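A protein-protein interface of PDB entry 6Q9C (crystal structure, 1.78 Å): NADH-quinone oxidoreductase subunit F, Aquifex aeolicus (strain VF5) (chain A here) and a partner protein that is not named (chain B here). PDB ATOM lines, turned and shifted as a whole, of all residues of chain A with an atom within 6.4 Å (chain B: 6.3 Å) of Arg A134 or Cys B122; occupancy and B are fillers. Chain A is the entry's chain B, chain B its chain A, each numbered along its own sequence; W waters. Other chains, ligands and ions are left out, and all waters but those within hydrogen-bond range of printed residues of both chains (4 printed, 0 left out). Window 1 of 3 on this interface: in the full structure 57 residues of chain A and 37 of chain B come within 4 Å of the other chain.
SG of Cys B126 sits close to N of Gly A98, 3.3 Å away.
O of Ala A176 is in hydrogen-bond range of N of Met B67, at 2.9 Å.
N of Gly A98 sits close to SG of Cys B122 (3.7 Å).
O of Cys B122 lies within hydrogen-bond range of NH2 of Arg A134, at 2.9 Å.
The guanidinium group of Arg A134 is in salt-bridge range of the side-chain carboxylate of Glu A136 (3.0 Å).
The side-chain hydroxyl (OG1) of Thr A99 lies within hydrogen-bond range of the backbone carbonyl oxygen (O) of Pro A97, at 3.4 Å.
The backbone carbonyl oxygen (O) of Gly A135 sits at hydrogen-bond distance from the guanidinium group (NH2) of Arg A174 (2.8 Å).
OE1 of Glu A94 lies within hydrogen-bond range of OH of Tyr A137 (2.7 Å).
The backbone NH of Gly A135 lies close to the backbone carbonyl oxygen of Gly A175.
O of Glu A94 is in hydrogen-bond range of NH1 of Arg A134 (2.9 Å).
Among the printed residues, merely in contact across the chains: Glu A96 with Cys B122 (3.97 Å), Pro A97 with Ile B84 (3.9 Å), Pro A97 with Cys B122 (3.7 Å), Thr A99 with Gly B124 (3.5 Å), Thr A99 with Cys B126 (3.98 Å), Arg A134 with Leu B123 (3.6 Å), Arg A134 with Gly B124 (3.6 Å), Gly A135 with Met B67 (3.7 Å), Glu A136 with Met B67 (3.98 Å), Glu A136 with Leu B123 (3.9 Å), Tyr A137 with Leu B123 (3.5 Å), Tyr A137 with Gly B124 (3.5 Å), Gly A177 with Met B67 (3.8 Å) and Phe A340 with Gln B121 (3.6 Å).
Of the printed residues of chain B, Gly A98 touches Cys B122 (3.7 Å) and Cys B126 (3.2 Å).
Of chain B, only Cys B122 (2.9 Å), Leu B123 (3.6 Å) and Gly B124 (3.6 Å) come within 4 Å of Arg A134.
Printed residues of chain B within 4 Å of Gly A177: Met B67.
Of chain A, only Glu A96 (3.97 Å), Pro A97 (3.7 Å), Gly A98 (3.7 Å) and Arg A134 (2.9 Å) come within 4 Å of Cys B122.
Printed residues of chain B that touch a printed residue of chain A: Met B67, Ile B84, Gln B121, Cys B122, Leu B123, Gly B124 and Cys B126.
Of the 22 printed residues of chain A, 11 touch a printed residue of chain B.
Hydrophobic or aromatic side chains of chain A within 4 Å of the printed part of chain B: Pro A97, Tyr A137 and Phe A340.
Among the printed residues, 18 pairs touch across the chains.
Water W1 bridges O of Leu B123 and O of Glu A136.
Water W2 bridges O of Ser A95 (2.7 Å) and O of Cys B122 (2.8 Å).
Water W4 lies within hydrogen-bond range of the backbone carbonyl oxygen of Gln B121 (2.8 Å), the guanidinium group of Arg A134 (3.1 Å) and the side-chain carboxylate of Glu A136 (3.3 Å).
Water W3 lies within hydrogen-bond range of O of Glu A96, O of Thr A99, NH1 of Arg A134 and N of Gly B124.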
ATOM      1  N   ALA A  92      -4.575 -15.724  13.171  1.00  0.00           N
ATOM      2  CA  ALA A  92      -5.889 -15.090  12.906  1.00  0.00           C
ATOM      3  C   ALA A  92      -5.760 -14.155  11.698  1.00  0.00           C
ATOM      4  O   ALA A  92      -6.448 -13.122  11.645  1.00  0.00           O
ATOM      5  CB  ALA A  92      -6.376 -14.358  14.137  1.00  0.00           C
ATOM      6  N   ASP A  93      -4.901 -14.495  10.735  1.00  0.00           N
ATOM      7  CA  ASP A  93      -4.705 -13.615   9.555  1.00  0.00           C
ATOM      8  C   ASP A  93      -5.806 -13.835   8.505  1.00  0.00           C
ATOM      9  O   ASP A  93      -5.897 -12.981   7.607  1.00  0.00           O
ATOM     10  CB  ASP A  93      -3.330 -13.782   8.915  1.00  0.00           C
ATOM     11  CG  ASP A  93      -2.987 -12.569   8.072  1.00  0.00           C
ATOM     12  OD1 ASP A  93      -2.926 -11.465   8.655  1.00  0.00           O
ATOM     13  OD2 ASP A  93      -2.839 -12.724   6.830  1.00  0.00           O
ATOM     14  N   GLU A  94      -6.554 -14.945   8.587  1.00  0.00           N
ATOM     15  CA  GLU A  94      -7.645 -15.368   7.664  1.00  0.00           C
ATOM     16  C   GLU A  94      -7.865 -14.370   6.518  1.00  0.00           C
ATOM     17  O   GLU A  94      -8.658 -13.432   6.689  1.00  0.00           O
ATOM     18  CB  GLU A  94      -8.947 -15.522   8.449  1.00  0.00           C
ATOM     19  CG  GLU A  94     -10.127 -15.916   7.586  1.00  0.00           C
ATOM     20  CD  GLU A  94     -11.315 -16.358   8.416  1.00  0.00           C
ATOM     21  OE1 GLU A  94     -11.916 -15.491   9.090  1.00  0.00           O
ATOM     22  OE2 GLU A  94     -11.606 -17.564   8.410  1.00  0.00           O
ATOM     23  N   SER A  95      -7.207 -14.577   5.375  1.00  0.00           N
ATOM     24  CA  SER A  95      -7.313 -13.681   4.195  1.00  0.00           C
ATOM     25  C   SER A  95      -7.526 -14.459   2.886  1.00  0.00           C
ATOM     26  O   SER A  95      -7.558 -13.797   1.841  1.00  0.00           O
ATOM     27  CB  SER A  95      -6.102 -12.788   4.109  1.00  0.00           C
ATOM     28  OG  SER A  95      -6.042 -11.925   5.237  1.00  0.00           O
ATOM     29  N   GLU A  96      -7.723 -15.784   2.925  1.00  0.00           N
ATOM     30  CA  GLU A  96      -8.077 -16.582   1.718  1.00  0.00           C
ATOM     31  C   GLU A  96      -9.429 -16.106   1.186  1.00  0.00           C
ATOM     32  O   GLU A  96     -10.384 -15.986   1.949  1.00  0.00           O
ATOM     33  CB  GLU A  96      -8.153 -18.075   2.041  1.00  0.00           C
ATOM     34  CG  GLU A  96      -8.347 -18.966   0.828  1.00  0.00           C
ATOM     35  CD  GLU A  96      -7.115 -19.148  -0.041  1.00  0.00           C
ATOM     36  OE1 GLU A  96      -6.128 -18.394   0.154  1.00  0.00           O
ATOM     37  OE2 GLU A  96      -7.147 -20.046  -0.914  1.00  0.00           O
ATOM     38  N   PRO A  97      -9.569 -15.806  -0.125  1.00  0.00           N
ATOM     39  CA  PRO A  97     -10.881 -15.504  -0.698  1.00  0.00           C
ATOM     40  C   PRO A  97     -11.946 -16.532  -0.286  1.00  0.00           C
ATOM     41  O   PRO A  97     -11.659 -17.716  -0.274  1.00  0.00           O
ATOM     42  CB  PRO A  97     -10.592 -15.500  -2.207  1.00  0.00           C
ATOM     43  CG  PRO A  97      -9.180 -14.973  -2.273  1.00  0.00           C
ATOM     44  CD  PRO A  97      -8.483 -15.646  -1.108  1.00  0.00           C
ATOM     45  N   GLY A  98     -13.124 -16.047   0.117  1.00  0.00           N
ATOM     46  CA  GLY A  98     -14.272 -16.882   0.512  1.00  0.00           C
ATOM     47  C   GLY A  98     -14.208 -17.344   1.959  1.00  0.00           C
ATOM     48  O   GLY A  98     -15.159 -18.025   2.385  1.00  0.00           O
ATOM     49  N   THR A  99     -13.129 -17.042   2.687  1.00  0.00           N
ATOM     50  CA  THR A  99     -12.838 -17.646   4.017  1.00  0.00           C
ATOM     51  C   THR A  99     -13.157 -16.641   5.130  1.00  0.00           C
ATOM     52  O   THR A  99     -12.489 -15.588   5.236  1.00  0.00           O
ATOM     53  CB  THR A  99     -11.414 -18.209   4.065  1.00  0.00           C
ATOM     54  OG1 THR A  99     -11.214 -18.915   2.839  1.00  0.00           O
ATOM     55  CG2 THR A  99     -11.198 -19.150   5.229  1.00  0.00           C
ATOM     56  N   TYR A 132      -1.931 -13.103  16.010  1.00  0.00           N
ATOM     57  CA  TYR A 132      -1.697 -12.223  14.842  1.00  0.00           C
ATOM     58  C   TYR A 132      -3.016 -12.145  14.081  1.00  0.00           C
ATOM     59  O   TYR A 132      -3.392 -13.133  13.429  1.00  0.00           O
ATOM     60  CB  TYR A 132      -0.548 -12.742  13.983  1.00  0.00           C
ATOM     61  CG  TYR A 132      -0.095 -11.768  12.930  1.00  0.00           C
ATOM     62  CD1 TYR A 132      -0.726 -11.699  11.696  1.00  0.00           C
ATOM     63  CD2 TYR A 132       0.960 -10.902  13.167  1.00  0.00           C
ATOM     64  CE1 TYR A 132      -0.308 -10.809  10.719  1.00  0.00           C
ATOM     65  CE2 TYR A 132       1.394 -10.010  12.197  1.00  0.00           C
ATOM     66  CZ  TYR A 132       0.762  -9.967  10.966  1.00  0.00           C
ATOM     67  OH  TYR A 132       1.183  -9.087  10.007  1.00  0.00           O
ATOM     68  N   ILE A 133      -3.737 -11.040  14.247  1.00  0.00           N
ATOM     69  CA  ILE A 133      -5.042 -10.826  13.563  1.00  0.00           C
ATOM     70  C   ILE A 133      -4.824  -9.837  12.419  1.00  0.00           C
ATOM     71  O   ILE A 133      -4.112  -8.834  12.621  1.00  0.00           O
ATOM     72  CB  ILE A 133      -6.153 -10.401  14.545  1.00  0.00           C
ATOM     73  CG1 ILE A 133      -7.520 -10.388  13.854  1.00  0.00           C
ATOM     74  CG2 ILE A 133      -5.842  -9.075  15.223  1.00  0.00           C
ATOM     75  CD1 ILE A 133      -8.691 -10.246  14.801  1.00  0.00           C
ATOM     76  N   ARG A 134      -5.397 -10.137  11.252  1.00  0.00           N
ATOM     77  CA  ARG A 134      -5.274  -9.278  10.044  1.00  0.00           C
ATOM     78  C   ARG A 134      -5.767  -7.864  10.373  1.00  0.00           C
ATOM     79  O   ARG A 134      -6.713  -7.718  11.187  1.00  0.00           O
ATOM     80  CB  ARG A 134      -6.041  -9.873   8.859  1.00  0.00           C
ATOM     81  CG  ARG A 134      -7.546  -9.974   9.067  1.00  0.00           C
ATOM     82  CD  ARG A 134      -8.257 -10.558   7.862  1.00  0.00           C
ATOM     83  NE  ARG A 134      -8.169  -9.708   6.685  1.00  0.00           N
ATOM     84  CZ  ARG A 134      -8.746  -9.962   5.512  1.00  0.00           C
ATOM     85  NH1 ARG A 134      -9.484 -11.046   5.351  1.00  0.00           N
ATOM     86  NH2 ARG A 134      -8.582  -9.121   4.506  1.00  0.00           N
ATOM     87  N   GLY A 135      -5.146  -6.857   9.753  1.00  0.00           N
ATOM     88  CA  GLY A 135      -5.476  -5.436   9.945  1.00  0.00           C
ATOM     89  C   GLY A 135      -6.941  -5.134   9.673  1.00  0.00           C
ATOM     90  O   GLY A 135      -7.477  -4.215  10.325  1.00  0.00           O
ATOM     91  N   GLU A 136      -7.565  -5.876   8.753  1.00  0.00           N
ATOM     92  CA  GLU A 136      -8.938  -5.603   8.247  1.00  0.00           C
ATOM     93  C   GLU A 136      -9.991  -6.225   9.177  1.00  0.00           C
ATOM     94  O   GLU A 136     -11.191  -6.107   8.847  1.00  0.00           O
ATOM     95  CB  GLU A 136      -9.101  -6.103   6.812  1.00  0.00           C
ATOM     96  CG  GLU A 136      -8.102  -5.501   5.834  1.00  0.00           C
ATOM     97  CD  GLU A 136      -6.786  -6.249   5.696  1.00  0.00           C
ATOM     98  OE1 GLU A 136      -6.533  -7.179   6.503  1.00  0.00           O
ATOM     99  OE2 GLU A 136      -6.020  -5.909   4.765  1.00  0.00           O
ATOM    100  N   TYR A 137      -9.575  -6.810  10.306  1.00  0.00           N
ATOM    101  CA  TYR A 137     -10.472  -7.289  11.393  1.00  0.00           C
ATOM    102  C   TYR A 137     -10.290  -6.408  12.634  1.00  0.00           C
ATOM    103  O   TYR A 137      -9.920  -6.901  13.704  1.00  0.00           O
ATOM    104  CB  TYR A 137     -10.181  -8.754  11.737  1.00  0.00           C
ATOM    105  CG  TYR A 137     -10.629  -9.826  10.771  1.00  0.00           C
ATOM    106  CD1 TYR A 137     -11.450  -9.570   9.678  1.00  0.00           C
ATOM    107  CD2 TYR A 137     -10.270 -11.144  11.003  1.00  0.00           C
ATOM    108  CE1 TYR A 137     -11.863 -10.586   8.827  1.00  0.00           C
ATOM    109  CE2 TYR A 137     -10.676 -12.169  10.165  1.00  0.00           C
ATOM    110  CZ  TYR A 137     -11.484 -11.893   9.075  1.00  0.00           C
ATOM    111  OH  TYR A 137     -11.884 -12.911   8.254  1.00  0.00           O
ATOM    112  N   PRO A 138     -10.545  -5.080  12.560  1.00  0.00           N
ATOM    113  CA  PRO A 138     -10.349  -4.204  13.716  1.00  0.00           C
ATOM    114  C   PRO A 138     -11.269  -4.563  14.893  1.00  0.00           C
ATOM    115  O   PRO A 138     -10.819  -4.504  16.021  1.00  0.00           O
ATOM    116  CB  PRO A 138     -10.656  -2.798  13.185  1.00  0.00           C
ATOM    117  CG  PRO A 138     -11.527  -3.037  11.968  1.00  0.00           C
ATOM    118  CD  PRO A 138     -11.027  -4.339  11.384  1.00  0.00           C
ATOM    119  N   TYR A 141      -9.890  -7.438  16.772  1.00  0.00           N
ATOM    120  CA  TYR A 141      -8.730  -6.969  17.572  1.00  0.00           C
ATOM    121  C   TYR A 141      -9.210  -6.411  18.920  1.00  0.00           C
ATOM    122  O   TYR A 141      -8.714  -6.850  19.977  1.00  0.00           O
ATOM    123  CB  TYR A 141      -7.910  -5.933  16.800  1.00  0.00           C
ATOM    124  CG  TYR A 141      -6.879  -5.238  17.647  1.00  0.00           C
ATOM    125  CD1 TYR A 141      -5.672  -5.851  17.940  1.00  0.00           C
ATOM    126  CD2 TYR A 141      -7.115  -3.981  18.177  1.00  0.00           C
ATOM    127  CE1 TYR A 141      -4.713  -5.229  18.719  1.00  0.00           C
ATOM    128  CE2 TYR A 141      -6.170  -3.346  18.968  1.00  0.00           C
ATOM    129  CZ  TYR A 141      -4.968  -3.977  19.247  1.00  0.00           C
ATOM    130  OH  TYR A 141      -4.036  -3.353  20.025  1.00  0.00           O
ATOM    131  N   ALA A 173      -1.178  -8.873  18.134  1.00  0.00           N
ATOM    132  CA  ALA A 173      -0.523  -8.126  17.042  1.00  0.00           C
ATOM    133  C   ALA A 173      -1.525  -7.969  15.896  1.00  0.00           C
ATOM    134  O   ALA A 173      -2.399  -8.839  15.737  1.00  0.00           O
ATOM    135  CB  ALA A 173       0.729  -8.838  16.591  1.00  0.00           C
ATOM    136  N   ARG A 174      -1.406  -6.879  15.142  1.00  0.00           N
ATOM    137  CA  ARG A 174      -2.282  -6.606  13.981  1.00  0.00           C
ATOM    138  C   ARG A 174      -1.451  -6.640  12.704  1.00  0.00           C
ATOM    139  O   ARG A 174      -0.344  -6.072  12.703  1.00  0.00           O
ATOM    140  CB  ARG A 174      -2.955  -5.239  14.096  1.00  0.00           C
ATOM    141  CG  ARG A 174      -3.992  -5.146  15.199  1.00  0.00           C
ATOM    142  CD  ARG A 174      -4.668  -3.790  15.162  1.00  0.00           C
ATOM    143  NE  ARG A 174      -5.576  -3.671  14.028  1.00  0.00           N
ATOM    144  CZ  ARG A 174      -6.097  -2.533  13.579  1.00  0.00           C
ATOM    145  NH1 ARG A 174      -5.809  -1.381  14.160  1.00  0.00           N
ATOM    146  NH2 ARG A 174      -6.904  -2.553  12.535  1.00  0.00           N
ATOM    147  N   GLY A 175      -2.003  -7.262  11.666  1.00  0.00           N
ATOM    148  CA  GLY A 175      -1.514  -7.153  10.281  1.00  0.00           C
ATOM    149  C   GLY A 175      -1.785  -5.770   9.721  1.00  0.00           C
ATOM    150  O   GLY A 175      -2.376  -4.927  10.439  1.00  0.00           O
ATOM    151  N   ALA A 176      -1.369  -5.520   8.484  1.00  0.00           N
ATOM    152  CA  ALA A 176      -1.547  -4.211   7.819  1.00  0.00           C
ATOM    153  C   ALA A 176      -1.724  -4.386   6.305  1.00  0.00           C
ATOM    154  O   ALA A 176      -1.343  -3.468   5.578  1.00  0.00           O
ATOM    155  CB  ALA A 176      -0.388  -3.316   8.172  1.00  0.00           C
ATOM    156  N   GLY A 177      -2.349  -5.488   5.863  1.00  0.00           N
ATOM    157  CA  GLY A 177      -2.909  -5.627   4.501  1.00  0.00           C
ATOM    158  C   GLY A 177      -2.236  -6.673   3.620  1.00  0.00           C
ATOM    159  O   GLY A 177      -2.590  -6.727   2.421  1.00  0.00           O
ATOM    160  N   PHE A 340      -5.792 -11.637  -7.576  1.00  0.00           N
ATOM    161  CA  PHE A 340      -5.499 -11.861  -6.140  1.00  0.00           C
ATOM    162  C   PHE A 340      -4.008 -12.177  -5.968  1.00  0.00           C
ATOM    163  O   PHE A 340      -3.331 -11.474  -5.199  1.00  0.00           O
ATOM    164  CB  PHE A 340      -6.372 -12.975  -5.567  1.00  0.00           C
ATOM    165  CG  PHE A 340      -6.151 -13.175  -4.095  1.00  0.00           C
ATOM    166  CD1 PHE A 340      -6.721 -12.307  -3.178  1.00  0.00           C
ATOM    167  CD2 PHE A 340      -5.348 -14.202  -3.636  1.00  0.00           C
ATOM    168  CE1 PHE A 340      -6.513 -12.487  -1.820  1.00  0.00           C
ATOM    169  CE2 PHE A 340      -5.142 -14.379  -2.278  1.00  0.00           C
ATOM    170  CZ  PHE A 340      -5.710 -13.512  -1.378  1.00  0.00           C
ATOM    171  N   MET B  67      -2.272  -1.378   3.752  1.00  0.00           N
ATOM    172  CA  MET B  67      -3.233  -0.539   4.519  1.00  0.00           C
ATOM    173  C   MET B  67      -2.664   0.869   4.731  1.00  0.00           C
ATOM    174  O   MET B  67      -3.472   1.810   4.858  1.00  0.00           O
ATOM    175  CB  MET B  67      -3.580  -1.175   5.866  1.00  0.00           C
ATOM    176  CG  MET B  67      -4.511  -2.353   5.715  1.00  0.00           C
ATOM    177  SD  MET B  67      -5.161  -2.950   7.290  1.00  0.00           S
ATOM    178  CE  MET B  67      -6.325  -1.652   7.701  1.00  0.00           C
ATOM    179  N   CYS B  81     -14.228  -4.243  -1.452  1.00  0.00           N
ATOM    180  CA  CYS B  81     -13.686  -5.557  -1.859  1.00  0.00           C
ATOM    181  C   CYS B  81     -13.897  -5.755  -3.363  1.00  0.00           C
ATOM    182  O   CYS B  81     -15.046  -5.648  -3.819  1.00  0.00           O
ATOM    183  CB  CYS B  81     -14.331  -6.697  -1.092  1.00  0.00           C
ATOM    184  SG  CYS B  81     -13.632  -8.288  -1.590  1.00  0.00           S
ATOM    185  N   VAL B  82     -12.817  -6.030  -4.094  1.00  0.00           N
ATOM    186  CA  VAL B  82     -12.837  -6.271  -5.566  1.00  0.00           C
ATOM    187  C   VAL B  82     -12.474  -7.733  -5.856  1.00  0.00           C
ATOM    188  O   VAL B  82     -12.187  -8.036  -7.035  1.00  0.00           O
ATOM    189  CB  VAL B  82     -11.896  -5.297  -6.307  1.00  0.00           C
ATOM    190  CG1 VAL B  82     -12.359  -3.858  -6.143  1.00  0.00           C
ATOM    191  CG2 VAL B  82     -10.440  -5.450  -5.880  1.00  0.00           C
ATOM    192  N   SER B  83     -12.505  -8.615  -4.851  1.00  0.00           N
ATOM    193  CA  SER B  83     -12.103 -10.042  -4.994  1.00  0.00           C
ATOM    194  C   SER B  83     -13.284 -10.869  -5.523  1.00  0.00           C
ATOM    195  O   SER B  83     -14.389 -10.311  -5.669  1.00  0.00           O
ATOM    196  CB  SER B  83     -11.556 -10.606  -3.706  1.00  0.00           C
ATOM    197  OG  SER B  83     -10.199 -10.233  -3.550  1.00  0.00           O
ATOM    198  N   ILE B  84     -13.041 -12.156  -5.771  1.00  0.00           N
ATOM    199  CA  ILE B  84     -13.935 -13.072  -6.547  1.00  0.00           C
ATOM    200  C   ILE B  84     -15.389 -12.979  -6.053  1.00  0.00           C
ATOM    201  O   ILE B  84     -16.267 -12.735  -6.897  1.00  0.00           O
ATOM    202  CB  ILE B  84     -13.396 -14.522  -6.549  1.00  0.00           C
ATOM    203  CG1 ILE B  84     -14.304 -15.481  -7.326  1.00  0.00           C
ATOM    204  CG2 ILE B  84     -13.150 -15.040  -5.143  1.00  0.00           C
ATOM    205  CD1 ILE B  84     -14.422 -15.177  -8.788  1.00  0.00           C
ATOM    206  N   VAL B  85     -15.673 -13.174  -4.763  1.00  0.00           N
ATOM    207  CA  VAL B  85     -17.088 -13.338  -4.307  1.00  0.00           C
ATOM    208  C   VAL B  85     -17.814 -11.993  -4.423  1.00  0.00           C
ATOM    209  O   VAL B  85     -18.908 -11.961  -5.004  1.00  0.00           O
ATOM    210  CB  VAL B  85     -17.208 -13.944  -2.898  1.00  0.00           C
ATOM    211  CG1 VAL B  85     -18.657 -14.278  -2.573  1.00  0.00           C
ATOM    212  CG2 VAL B  85     -16.328 -15.180  -2.742  1.00  0.00           C
ATOM    213  N   VAL B 120      -9.733  -3.075  -2.264  1.00  0.00           N
ATOM    214  CA  VAL B 120      -9.018  -4.051  -1.391  1.00  0.00           C
ATOM    215  C   VAL B 120      -9.372  -5.468  -1.838  1.00  0.00           C
ATOM    216  O   VAL B 120     -10.426  -5.660  -2.486  1.00  0.00           O
ATOM    217  CB  VAL B 120      -9.335  -3.848   0.105  1.00  0.00           C
ATOM    218  CG1 VAL B 120      -8.905  -2.473   0.594  1.00  0.00           C
ATOM    219  CG2 VAL B 120     -10.800  -4.093   0.416  1.00  0.00           C
ATOM    220  N   GLN B 121      -8.520  -6.422  -1.470  1.00  0.00           N
ATOM    221  CA  GLN B 121      -8.750  -7.871  -1.683  1.00  0.00           C
ATOM    222  C   GLN B 121      -9.681  -8.380  -0.580  1.00  0.00           C
ATOM    223  O   GLN B 121      -9.985  -7.610   0.345  1.00  0.00           O
ATOM    224  CB  GLN B 121      -7.427  -8.634  -1.702  1.00  0.00           C
ATOM    225  CG  GLN B 121      -6.400  -8.053  -2.670  1.00  0.00           C
ATOM    226  CD  GLN B 121      -6.869  -8.068  -4.103  1.00  0.00           C
ATOM    227  OE1 GLN B 121      -7.344  -9.081  -4.601  1.00  0.00           O
ATOM    228  NE2 GLN B 121      -6.728  -6.941  -4.787  1.00  0.00           N
ATOM    229  N   CYS B 122     -10.128  -9.624  -0.719  1.00  0.00           N
ATOM    230  CA  CYS B 122     -11.170 -10.269   0.116  1.00  0.00           C
ATOM    231  C   CYS B 122     -11.063  -9.806   1.573  1.00  0.00           C
ATOM    232  O   CYS B 122      -9.982  -9.977   2.169  1.00  0.00           O
ATOM    233  CB  CYS B 122     -11.037 -11.782   0.067  1.00  0.00           C
ATOM    234  SG  CYS B 122     -12.279 -12.605   1.090  1.00  0.00           S
ATOM    235  N   LEU B 123     -12.162  -9.276   2.117  1.00  0.00           N
ATOM    236  CA  LEU B 123     -12.244  -8.735   3.503  1.00  0.00           C
ATOM    237  C   LEU B 123     -12.734  -9.805   4.488  1.00  0.00           C
ATOM    238  O   LEU B 123     -12.957  -9.452   5.667  1.00  0.00           O
ATOM    239  CB  LEU B 123     -13.184  -7.526   3.496  1.00  0.00           C
ATOM    240  CG  LEU B 123     -12.607  -6.258   2.869  1.00  0.00           C
ATOM    241  CD1 LEU B 123     -13.700  -5.227   2.636  1.00  0.00           C
ATOM    242  CD2 LEU B 123     -11.507  -5.688   3.747  1.00  0.00           C
ATOM    243  N   GLY B 124     -12.878 -11.061   4.054  1.00  0.00           N
ATOM    244  CA  GLY B 124     -13.329 -12.156   4.936  1.00  0.00           C
ATOM    245  C   GLY B 124     -14.736 -11.913   5.468  1.00  0.00           C
ATOM    246  O   GLY B 124     -14.966 -12.167   6.666  1.00  0.00           O
ATOM    247  N   ALA B 125     -15.664 -11.453   4.621  1.00  0.00           N
ATOM    248  CA  ALA B 125     -17.109 -11.350   4.957  1.00  0.00           C
ATOM    249  C   ALA B 125     -17.962 -11.808   3.764  1.00  0.00           C
ATOM    250  O   ALA B 125     -19.064 -11.257   3.558  1.00  0.00           O
ATOM    251  CB  ALA B 125     -17.430  -9.934   5.369  1.00  0.00           C
ATOM    252  N   CYS B 126     -17.494 -12.820   3.033  1.00  0.00           N
ATOM    253  CA  CYS B 126     -17.891 -13.086   1.622  1.00  0.00           C
ATOM    254  C   CYS B 126     -19.373 -13.478   1.536  1.00  0.00           C
ATOM    255  O   CYS B 126     -19.987 -13.187   0.512  1.00  0.00           O
ATOM    256  CB  CYS B 126     -17.008 -14.158   1.001  1.00  0.00           C
ATOM    257  SG  CYS B 126     -15.249 -13.934   1.379  1.00  0.00           S
HETATM  258  O   HOH W   1     -12.978  -7.347   7.229  1.00  0.00           O
HETATM  259  O   HOH W   2      -7.666 -11.159   1.232  1.00  0.00           O
HETATM  260  O   HOH W   3     -10.650 -13.535   3.801  1.00  0.00           O
HETATM  261  O   HOH W   4      -8.215  -6.829   2.418  1.00  0.00           O
